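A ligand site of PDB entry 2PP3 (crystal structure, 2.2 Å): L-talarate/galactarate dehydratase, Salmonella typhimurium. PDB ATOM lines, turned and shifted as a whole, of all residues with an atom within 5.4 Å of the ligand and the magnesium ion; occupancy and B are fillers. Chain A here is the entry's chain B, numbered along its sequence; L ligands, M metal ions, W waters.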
ATOM      1  N   VAL A  44      -8.135  -6.500  19.126  1.00  0.00           N
ATOM      2  CA  VAL A  44      -8.509  -5.577  18.071  1.00  0.00           C
ATOM      3  C   VAL A  44      -9.877  -4.931  18.310  1.00  0.00           C
ATOM      4  O   VAL A  44     -10.827  -5.602  18.716  1.00  0.00           O
ATOM      5  CB  VAL A  44      -8.528  -6.298  16.704  1.00  0.00           C
ATOM      6  CG1 VAL A  44      -8.946  -5.335  15.609  1.00  0.00           C
ATOM      7  CG2 VAL A  44      -7.158  -6.875  16.422  1.00  0.00           C
ATOM      8  N   SER A  45      -9.970  -3.638  18.050  1.00  0.00           N
ATOM      9  CA  SER A  45     -11.234  -2.945  18.230  1.00  0.00           C
ATOM     10  C   SER A  45     -11.459  -1.824  17.219  1.00  0.00           C
ATOM     11  O   SER A  45     -10.615  -0.947  17.058  1.00  0.00           O
ATOM     12  CB  SER A  45     -11.331  -2.388  19.658  1.00  0.00           C
ATOM     13  OG  SER A  45     -10.352  -1.393  19.878  1.00  0.00           O
ATOM     14  N   ASP A  46     -12.587  -1.900  16.520  1.00  0.00           N
ATOM     15  CA  ASP A  46     -12.958  -0.868  15.554  1.00  0.00           C
ATOM     16  C   ASP A  46     -14.056  -0.033  16.213  1.00  0.00           C
ATOM     17  O   ASP A  46     -14.263  -0.139  17.427  1.00  0.00           O
ATOM     18  CB  ASP A  46     -13.450  -1.478  14.233  1.00  0.00           C
ATOM     19  CG  ASP A  46     -14.509  -2.551  14.445  1.00  0.00           C
ATOM     20  OD1 ASP A  46     -15.417  -2.363  15.275  1.00  0.00           O
ATOM     21  OD2 ASP A  46     -14.444  -3.581  13.748  1.00  0.00           O
ATOM     22  N   LYS A  48     -17.128  -0.446  16.329  1.00  0.00           N
ATOM     23  CA  LYS A  48     -18.148  -1.270  16.977  1.00  0.00           C
ATOM     24  C   LYS A  48     -17.860  -1.441  18.470  1.00  0.00           C
ATOM     25  O   LYS A  48     -18.786  -1.666  19.267  1.00  0.00           O
ATOM     26  CB  LYS A  48     -18.218  -2.646  16.300  1.00  0.00           C
ATOM     27  CG  LYS A  48     -18.799  -2.602  14.885  1.00  0.00           C
ATOM     28  CD  LYS A  48     -18.930  -3.998  14.277  1.00  0.00           C
ATOM     29  CE  LYS A  48     -17.587  -4.553  13.785  1.00  0.00           C
ATOM     30  NZ  LYS A  48     -16.587  -4.789  14.862  1.00  0.00           N
ATOM     31  N   GLN A  54     -19.812  -3.909  20.778  1.00  0.00           N
ATOM     32  CA  GLN A  54     -19.088  -5.162  20.985  1.00  0.00           C
ATOM     33  C   GLN A  54     -17.840  -4.983  21.844  1.00  0.00           C
ATOM     34  O   GLN A  54     -17.433  -3.853  22.155  1.00  0.00           O
ATOM     35  CB  GLN A  54     -18.655  -5.771  19.648  1.00  0.00           C
ATOM     36  CG  GLN A  54     -19.740  -5.998  18.630  1.00  0.00           C
ATOM     37  CD  GLN A  54     -19.170  -6.470  17.301  1.00  0.00           C
ATOM     38  OE1 GLN A  54     -18.246  -5.855  16.749  1.00  0.00           O
ATOM     39  NE2 GLN A  54     -19.711  -7.556  16.766  1.00  0.00           N
ATOM     40  N   LEU A  57     -11.825  -7.711  19.808  1.00  0.00           N
ATOM     41  CA  LEU A  57     -11.586  -9.020  19.201  1.00  0.00           C
ATOM     42  C   LEU A  57     -10.278  -9.592  19.750  1.00  0.00           C
ATOM     43  O   LEU A  57      -9.247  -8.922  19.723  1.00  0.00           O
ATOM     44  CB  LEU A  57     -11.493  -8.862  17.681  1.00  0.00           C
ATOM     45  CG  LEU A  57     -11.419 -10.140  16.844  1.00  0.00           C
ATOM     46  CD1 LEU A  57     -12.691 -10.947  16.996  1.00  0.00           C
ATOM     47  CD2 LEU A  57     -11.210  -9.758  15.385  1.00  0.00           C
ATOM     48  N   LYS A  82     -15.639 -14.044  13.434  1.00  0.00           N
ATOM     49  CA  LYS A  82     -15.029 -13.064  14.317  1.00  0.00           C
ATOM     50  C   LYS A  82     -16.087 -12.855  15.397  1.00  0.00           C
ATOM     51  O   LYS A  82     -17.096 -12.201  15.161  1.00  0.00           O
ATOM     52  CB  LYS A  82     -14.733 -11.762  13.577  1.00  0.00           C
ATOM     53  CG  LYS A  82     -13.590 -11.867  12.587  1.00  0.00           C
ATOM     54  CD  LYS A  82     -13.312 -10.519  11.935  1.00  0.00           C
ATOM     55  CE  LYS A  82     -12.206 -10.628  10.889  1.00  0.00           C
ATOM     56  NZ  LYS A  82     -11.955  -9.318  10.218  1.00  0.00           N
ATOM     57  N   ARG A  83     -15.842 -13.447  16.554  1.00  0.00           N
ATOM     58  CA  ARG A  83     -16.739 -13.415  17.708  1.00  0.00           C
ATOM     59  C   ARG A  83     -17.648 -14.628  17.601  1.00  0.00           C
ATOM     60  O   ARG A  83     -17.382 -15.512  16.782  1.00  0.00           O
ATOM     61  CB  ARG A  83     -17.538 -12.094  17.777  1.00  0.00           C
ATOM     62  CG  ARG A  83     -16.624 -10.890  18.029  1.00  0.00           C
ATOM     63  CD  ARG A  83     -17.384  -9.597  18.293  1.00  0.00           C
ATOM     64  NE  ARG A  83     -16.481  -8.483  18.589  1.00  0.00           N
ATOM     65  CZ  ARG A  83     -15.745  -7.846  17.687  1.00  0.00           C
ATOM     66  NH1 ARG A  83     -15.797  -8.191  16.398  1.00  0.00           N
ATOM     67  NH2 ARG A  83     -14.943  -6.860  18.068  1.00  0.00           N
ATOM     68  N   TYR A 165      -4.300  -3.512  -0.212  1.00  0.00           N
ATOM     69  CA  TYR A 165      -4.238  -2.483   0.819  1.00  0.00           C
ATOM     70  C   TYR A 165      -4.258  -3.173   2.187  1.00  0.00           C
ATOM     71  O   TYR A 165      -4.810  -4.266   2.327  1.00  0.00           O
ATOM     72  CB  TYR A 165      -5.424  -1.506   0.677  1.00  0.00           C
ATOM     73  CG  TYR A 165      -6.764  -2.053   1.147  1.00  0.00           C
ATOM     74  CD1 TYR A 165      -7.153  -1.940   2.483  1.00  0.00           C
ATOM     75  CD2 TYR A 165      -7.637  -2.681   0.261  1.00  0.00           C
ATOM     76  CE1 TYR A 165      -8.374  -2.449   2.924  1.00  0.00           C
ATOM     77  CE2 TYR A 165      -8.864  -3.194   0.686  1.00  0.00           C
ATOM     78  CZ  TYR A 165      -9.223  -3.069   2.027  1.00  0.00           C
ATOM     79  OH  TYR A 165     -10.427  -3.581   2.469  1.00  0.00           O
ATOM     80  N   THR A 167      -5.216  -3.317   6.323  1.00  0.00           N
ATOM     81  CA  THR A 167      -6.225  -2.876   7.285  1.00  0.00           C
ATOM     82  C   THR A 167      -5.769  -3.049   8.723  1.00  0.00           C
ATOM     83  O   THR A 167      -6.023  -2.186   9.574  1.00  0.00           O
ATOM     84  CB  THR A 167      -7.540  -3.665   7.109  1.00  0.00           C
ATOM     85  OG1 THR A 167      -8.118  -3.370   5.829  1.00  0.00           O
ATOM     86  CG2 THR A 167      -8.549  -3.310   8.204  1.00  0.00           C
ATOM     87  N   PHE A 171      -6.358   0.259  12.943  1.00  0.00           N
ATOM     88  CA  PHE A 171      -7.518   0.116  13.827  1.00  0.00           C
ATOM     89  C   PHE A 171      -7.550   1.183  14.928  1.00  0.00           C
ATOM     90  O   PHE A 171      -6.545   1.835  15.215  1.00  0.00           O
ATOM     91  CB  PHE A 171      -7.543  -1.285  14.422  1.00  0.00           C
ATOM     92  CG  PHE A 171      -8.104  -2.321  13.481  1.00  0.00           C
ATOM     93  CD1 PHE A 171      -9.472  -2.390  13.252  1.00  0.00           C
ATOM     94  CD2 PHE A 171      -7.266  -3.208  12.826  1.00  0.00           C
ATOM     95  CE1 PHE A 171     -10.006  -3.339  12.362  1.00  0.00           C
ATOM     96  CE2 PHE A 171      -7.783  -4.160  11.938  1.00  0.00           C
ATOM     97  CZ  PHE A 171      -9.151  -4.229  11.709  1.00  0.00           C
ATOM     98  N   LYS A 195      -6.168   1.520   4.775  1.00  0.00           N
ATOM     99  CA  LYS A 195      -7.537   1.748   5.214  1.00  0.00           C
ATOM    100  C   LYS A 195      -7.506   2.125   6.689  1.00  0.00           C
ATOM    101  O   LYS A 195      -6.937   1.415   7.521  1.00  0.00           O
ATOM    102  CB  LYS A 195      -8.415   0.504   5.024  1.00  0.00           C
ATOM    103  CG  LYS A 195      -9.869   0.745   5.456  1.00  0.00           C
ATOM    104  CD  LYS A 195     -10.851  -0.258   4.870  1.00  0.00           C
ATOM    105  CE  LYS A 195     -10.738  -1.619   5.503  1.00  0.00           C
ATOM    106  NZ  LYS A 195     -11.672  -2.576   4.852  1.00  0.00           N
ATOM    107  N   ASP A 226     -13.120   3.208   6.955  1.00  0.00           N
ATOM    108  CA  ASP A 226     -14.155   2.233   7.279  1.00  0.00           C
ATOM    109  C   ASP A 226     -14.809   2.615   8.608  1.00  0.00           C
ATOM    110  O   ASP A 226     -14.169   2.576   9.658  1.00  0.00           O
ATOM    111  CB  ASP A 226     -13.469   0.876   7.393  1.00  0.00           C
ATOM    112  CG  ASP A 226     -14.439  -0.242   7.656  1.00  0.00           C
ATOM    113  OD1 ASP A 226     -15.632  -0.007   7.949  1.00  0.00           O
ATOM    114  OD2 ASP A 226     -13.969  -1.385   7.568  1.00  0.00           O
ATOM    115  N   ASN A 228     -17.482   1.027   9.872  1.00  0.00           N
ATOM    116  CA  ASN A 228     -18.109  -0.149  10.451  1.00  0.00           C
ATOM    117  C   ASN A 228     -19.535   0.063  10.975  1.00  0.00           C
ATOM    118  O   ASN A 228     -19.852  -0.311  12.111  1.00  0.00           O
ATOM    119  CB  ASN A 228     -17.220  -0.719  11.573  1.00  0.00           C
ATOM    120  CG  ASN A 228     -16.021  -1.486  11.020  1.00  0.00           C
ATOM    121  OD1 ASN A 228     -16.133  -2.652  10.609  1.00  0.00           O
ATOM    122  ND2 ASN A 228     -14.859  -0.843  11.002  1.00  0.00           N
ATOM    123  N   GLU A 252     -16.178   3.056   3.563  1.00  0.00           N
ATOM    124  CA  GLU A 252     -16.753   1.752   3.807  1.00  0.00           C
ATOM    125  C   GLU A 252     -17.765   1.712   4.954  1.00  0.00           C
ATOM    126  O   GLU A 252     -17.591   2.352   5.978  1.00  0.00           O
ATOM    127  CB  GLU A 252     -15.620   0.767   4.087  1.00  0.00           C
ATOM    128  CG  GLU A 252     -16.050  -0.668   4.180  1.00  0.00           C
ATOM    129  CD  GLU A 252     -14.872  -1.601   4.119  1.00  0.00           C
ATOM    130  OE1 GLU A 252     -13.863  -1.238   3.478  1.00  0.00           O
ATOM    131  OE2 GLU A 252     -14.968  -2.710   4.676  1.00  0.00           O
ATOM    132  N   GLU A 253     -18.835   0.939   4.750  1.00  0.00           N
ATOM    133  CA  GLU A 253     -19.878   0.776   5.751  1.00  0.00           C
ATOM    134  C   GLU A 253     -20.162   2.024   6.596  1.00  0.00           C
ATOM    135  O   GLU A 253     -19.994   2.012   7.812  1.00  0.00           O
ATOM    136  CB  GLU A 253     -19.525  -0.395   6.670  1.00  0.00           C
ATOM    137  CG  GLU A 253     -19.575  -1.760   5.990  1.00  0.00           C
ATOM    138  CD  GLU A 253     -19.921  -2.888   6.952  1.00  0.00           C
ATOM    139  OE1 GLU A 253     -19.061  -3.312   7.753  1.00  0.00           O
ATOM    140  OE2 GLU A 253     -21.081  -3.356   6.906  1.00  0.00           O
ATOM    141  N   GLU A 278     -19.664  -6.537   3.502  1.00  0.00           N
ATOM    142  CA  GLU A 278     -18.952  -7.554   4.246  1.00  0.00           C
ATOM    143  C   GLU A 278     -19.789  -8.332   5.267  1.00  0.00           C
ATOM    144  O   GLU A 278     -19.507  -9.496   5.539  1.00  0.00           O
ATOM    145  CB  GLU A 278     -17.746  -6.947   4.960  1.00  0.00           C
ATOM    146  CG  GLU A 278     -18.045  -6.427   6.350  1.00  0.00           C
ATOM    147  CD  GLU A 278     -16.832  -5.750   6.957  1.00  0.00           C
ATOM    148  OE1 GLU A 278     -16.264  -4.877   6.262  1.00  0.00           O
ATOM    149  OE2 GLU A 278     -16.464  -6.072   8.105  1.00  0.00           O
ATOM    150  N   GLN A 299     -18.592  -5.466  -1.476  1.00  0.00           N
ATOM    151  CA  GLN A 299     -17.619  -6.196  -0.677  1.00  0.00           C
ATOM    152  C   GLN A 299     -18.110  -7.523  -0.124  1.00  0.00           C
ATOM    153  O   GLN A 299     -18.344  -7.657   1.081  1.00  0.00           O
ATOM    154  CB  GLN A 299     -17.124  -5.304   0.466  1.00  0.00           C
ATOM    155  CG  GLN A 299     -16.568  -3.964  -0.013  1.00  0.00           C
ATOM    156  CD  GLN A 299     -16.040  -3.098   1.113  1.00  0.00           C
ATOM    157  OE1 GLN A 299     -16.794  -2.675   1.989  1.00  0.00           O
ATOM    158  NE2 GLN A 299     -14.740  -2.827   1.088  1.00  0.00           N
ATOM    159  N   ARG A 304     -18.453 -15.931   4.336  1.00  0.00           N
ATOM    160  CA  ARG A 304     -19.741 -15.466   4.857  1.00  0.00           C
ATOM    161  C   ARG A 304     -20.980 -15.666   3.988  1.00  0.00           C
ATOM    162  O   ARG A 304     -22.071 -15.846   4.522  1.00  0.00           O
ATOM    163  CB  ARG A 304     -19.650 -13.985   5.233  1.00  0.00           C
ATOM    164  CG  ARG A 304     -19.064 -13.739   6.616  1.00  0.00           C
ATOM    165  CD  ARG A 304     -18.945 -12.262   6.920  1.00  0.00           C
ATOM    166  NE  ARG A 304     -18.370 -12.043   8.239  1.00  0.00           N
ATOM    167  CZ  ARG A 304     -17.814 -10.894   8.621  1.00  0.00           C
ATOM    168  NH1 ARG A 304     -17.767  -9.863   7.788  1.00  0.00           N
ATOM    169  NH2 ARG A 304     -17.310 -10.774   9.844  1.00  0.00           N
ATOM    170  N   HIS A 328     -13.838  -8.901   1.205  1.00  0.00           N
ATOM    171  CA  HIS A 328     -13.468  -8.649   2.588  1.00  0.00           C
ATOM    172  C   HIS A 328     -12.729  -9.814   3.230  1.00  0.00           C
ATOM    173  O   HIS A 328     -13.153 -10.962   3.117  1.00  0.00           O
ATOM    174  CB  HIS A 328     -14.734  -8.324   3.394  1.00  0.00           C
ATOM    175  CG  HIS A 328     -14.544  -8.370   4.875  1.00  0.00           C
ATOM    176  ND1 HIS A 328     -14.729  -9.521   5.609  1.00  0.00           N
ATOM    177  CD2 HIS A 328     -14.161  -7.418   5.764  1.00  0.00           C
ATOM    178  CE1 HIS A 328     -14.486  -9.281   6.881  1.00  0.00           C
ATOM    179  NE2 HIS A 328     -14.133  -8.013   7.005  1.00  0.00           N
ATOM    180  N   GLU A 348      -7.863  -7.028   0.245  1.00  0.00           N
ATOM    181  CA  GLU A 348      -7.591  -6.587   1.600  1.00  0.00           C
ATOM    182  C   GLU A 348      -6.588  -7.464   2.326  1.00  0.00           C
ATOM    183  O   GLU A 348      -6.720  -8.687   2.374  1.00  0.00           O
ATOM    184  CB  GLU A 348      -8.902  -6.528   2.395  1.00  0.00           C
ATOM    185  CG  GLU A 348      -8.728  -6.248   3.879  1.00  0.00           C
ATOM    186  CD  GLU A 348     -10.056  -6.066   4.604  1.00  0.00           C
ATOM    187  OE1 GLU A 348     -10.972  -6.901   4.403  1.00  0.00           O
ATOM    188  OE2 GLU A 348     -10.172  -5.099   5.384  1.00  0.00           O
ATOM    189  N   PHE A 350      -4.388  -8.770   5.694  1.00  0.00           N
ATOM    190  CA  PHE A 350      -4.289  -9.026   7.127  1.00  0.00           C
ATOM    191  C   PHE A 350      -3.159 -10.047   7.217  1.00  0.00           C
ATOM    192  O   PHE A 350      -2.919 -10.777   6.255  1.00  0.00           O
ATOM    193  CB  PHE A 350      -5.568  -9.671   7.677  1.00  0.00           C
ATOM    194  CG  PHE A 350      -6.669  -8.713   8.006  1.00  0.00           C
ATOM    195  CD1 PHE A 350      -7.576  -8.303   7.036  1.00  0.00           C
ATOM    196  CD2 PHE A 350      -6.816  -8.239   9.308  1.00  0.00           C
ATOM    197  CE1 PHE A 350      -8.613  -7.432   7.360  1.00  0.00           C
ATOM    198  CE2 PHE A 350      -7.854  -7.371   9.646  1.00  0.00           C
ATOM    199  CZ  PHE A 350      -8.750  -6.968   8.661  1.00  0.00           C
ATOM    200  N   TRP A 352      -3.033 -11.950  10.077  1.00  0.00           N
ATOM    201  CA  TRP A 352      -3.657 -12.892  10.976  1.00  0.00           C
ATOM    202  C   TRP A 352      -3.627 -14.366  10.572  1.00  0.00           C
ATOM    203  O   TRP A 352      -3.271 -15.219  11.378  1.00  0.00           O
ATOM    204  CB  TRP A 352      -5.108 -12.483  11.228  1.00  0.00           C
ATOM    205  CG  TRP A 352      -5.245 -11.115  11.837  1.00  0.00           C
ATOM    206  CD1 TRP A 352      -4.243 -10.277  12.216  1.00  0.00           C
ATOM    207  CD2 TRP A 352      -6.471 -10.434  12.121  1.00  0.00           C
ATOM    208  NE1 TRP A 352      -4.759  -9.110  12.719  1.00  0.00           N
ATOM    209  CE2 TRP A 352      -6.127  -9.167  12.674  1.00  0.00           C
ATOM    210  CE3 TRP A 352      -7.829 -10.751  11.971  1.00  0.00           C
ATOM    211  CZ2 TRP A 352      -7.080  -8.243  13.070  1.00  0.00           C
ATOM    212  CZ3 TRP A 352      -8.780  -9.814  12.362  1.00  0.00           C
ATOM    213  CH2 TRP A 352      -8.405  -8.575  12.912  1.00  0.00           C
HETATM  214  O1  LIG L   1     -11.180  -5.527   7.633  1.00  0.00           O
HETATM  215  C1  LIG L   1     -12.288  -4.982   7.639  1.00  0.00           C
HETATM  216  O2  LIG L   1     -12.876  -4.587   6.606  1.00  0.00           O
HETATM  217  C2  LIG L   1     -13.005  -4.759   9.028  1.00  0.00           C
HETATM  218  O3  LIG L   1     -14.390  -4.403   8.853  1.00  0.00           O
HETATM  219  C3  LIG L   1     -12.928  -5.979   9.950  1.00  0.00           C
HETATM  220  O4  LIG L   1     -13.859  -6.963   9.505  1.00  0.00           O
HETATM  221  C4  LIG L   1     -13.240  -5.660  11.434  1.00  0.00           C
HETATM  222  O5  LIG L   1     -14.612  -5.225  11.547  1.00  0.00           O
HETATM  223  C5  LIG L   1     -13.045  -6.851  12.397  1.00  0.00           C
HETATM  224  O6  LIG L   1     -11.688  -7.314  12.284  1.00  0.00           O
HETATM  225  C6  LIG L   1     -13.315  -6.454  13.865  1.00  0.00           C
HETATM  226  O7  LIG L   1     -14.473  -6.697  14.305  1.00  0.00           O
HETATM  227  O8  LIG L   1     -12.388  -5.902  14.516  1.00  0.00           O
HETATM  228 MG    MG M   1     -14.728  -3.259   6.911  1.00  0.00          MG
HETATM  229  O   HOH W   1     -16.471  -7.900  12.852  1.00  0.00           O
HETATM  230  O   HOH W   2     -13.078  -4.975  16.687  1.00  0.00           O
HETATM  231  O   HOH W   3     -16.477  -8.116   9.828  1.00  0.00           O
HETATM  232  O   HOH W   4     -13.657  -5.010   3.525  1.00  0.00           O
HETATM  233  O   HOH W   5     -16.668  -2.547   7.627  1.00  0.00           O
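An oxygen (O1) of the ligand lies close to the side-chain carboxylate of Glu 348, 2.5 Å away.
NZ of Lys 48 is in salt-bridge range of O7 of the ligand, 2.9 Å away.
A ring nitrogen (NE2) of His 328 is in hydrogen-bond range of an oxygen (O4) of the ligand (2.7 Å).
OD1 of Asn 228 sits at hydrogen-bond distance from O5 of the ligand, 3.1 Å away.
NZ of Lys 82 sits at hydrogen-bond distance from O6 of the ligand, at 2.9 Å.
The side-chain amino group (NZ) of Lys 195 sits close to an oxygen (O2) of the ligand.
The side-chain carboxylate (OD2) of Asp 46 is in hydrogen-bond range of an oxygen (O5) of the ligand (2.8 Å).
The guanidinium group of Arg 83 is in salt-bridge range of an oxygen (O7) of the ligand, 2.9 Å away.
NZ of Lys 195 is in hydrogen-bond range of OH of Tyr 165.
The side-chain carboxylate of Asp 226 lies within hydrogen-bond range of the backbone NH of Asn 228 (2.9 Å).
The side-chain carboxylate of Glu 348 is in hydrogen-bond range of the side-chain hydroxyl of Thr 167, at 2.7 Å.
OD2 of Asp 226 sits close to NZ of Lys 195 (3.8 Å).
The guanidinium group (NH1) of Arg 83 lies close to the side-chain amide oxygen (OE1) of Gln 54, at 3.4 Å.
OE2 of Glu 348 sits at hydrogen-bond distance from OH of Tyr 165, at 3.3 Å.
The side-chain carboxylate (OE1) of Glu 252 lies within hydrogen-bond range of the side-chain amide nitrogen (NE2) of Gln 299, 3.0 Å away.
The side-chain carboxylate (OE1) of Glu 252 lies within salt-bridge range of the side-chain amino group (NZ) of Lys 195 (2.9 Å).
Residues that only touch the ligand: Phe 350 (3.0 Å), Thr 167 (3.5 Å), Trp 352 (3.6 Å), Val 44 (3.7 Å) and Leu 57 (3.98 Å).
The nearest printed residue that does not touch the ligand is Phe 171 (4.04 Å).
Lys 195 touches the magnesium ion (NZ to MG, 3.7 Å).
Of the 23 residues printed, 4 come within 4 Å of the magnesium ion.
The nearest printed residue that does not touch the magnesium ion is Asn 228 (4.002 Å).
The side-chain carboxylate (OD2) of Asp 226 binds the magnesium ion.
Water W5 is bound to the magnesium ion (2.2 Å).
The magnesium ion is bound by O3 of the ligand, at 2.3 Å.
O2 of the ligand binds the magnesium ion (2.3 Å).
OE2 of Glu 252 is bound to the magnesium ion (2.3 Å).
The magnesium ion is bound by OE1 of Glu 278 (2.3 Å).
The magnesium ion has six donor atoms within binding distance.
Water W2 lies within hydrogen-bond range of an oxygen (O8) of the ligand, the guanidinium group (NH2) of Arg 83, the backbone carbonyl oxygen (O) of Val 44 and the backbone NH (N) of Asp 46.
Water W3 lies within hydrogen-bond range of OE2 of Glu 278, NH2 of Arg 304 and O4 of the ligand.
Water W4 lies within hydrogen-bond range of OE1 of Glu 348 (3.4 Å), NZ of Lys 195 (3.4 Å) and NE2 of Gln 299 (3.4 Å).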
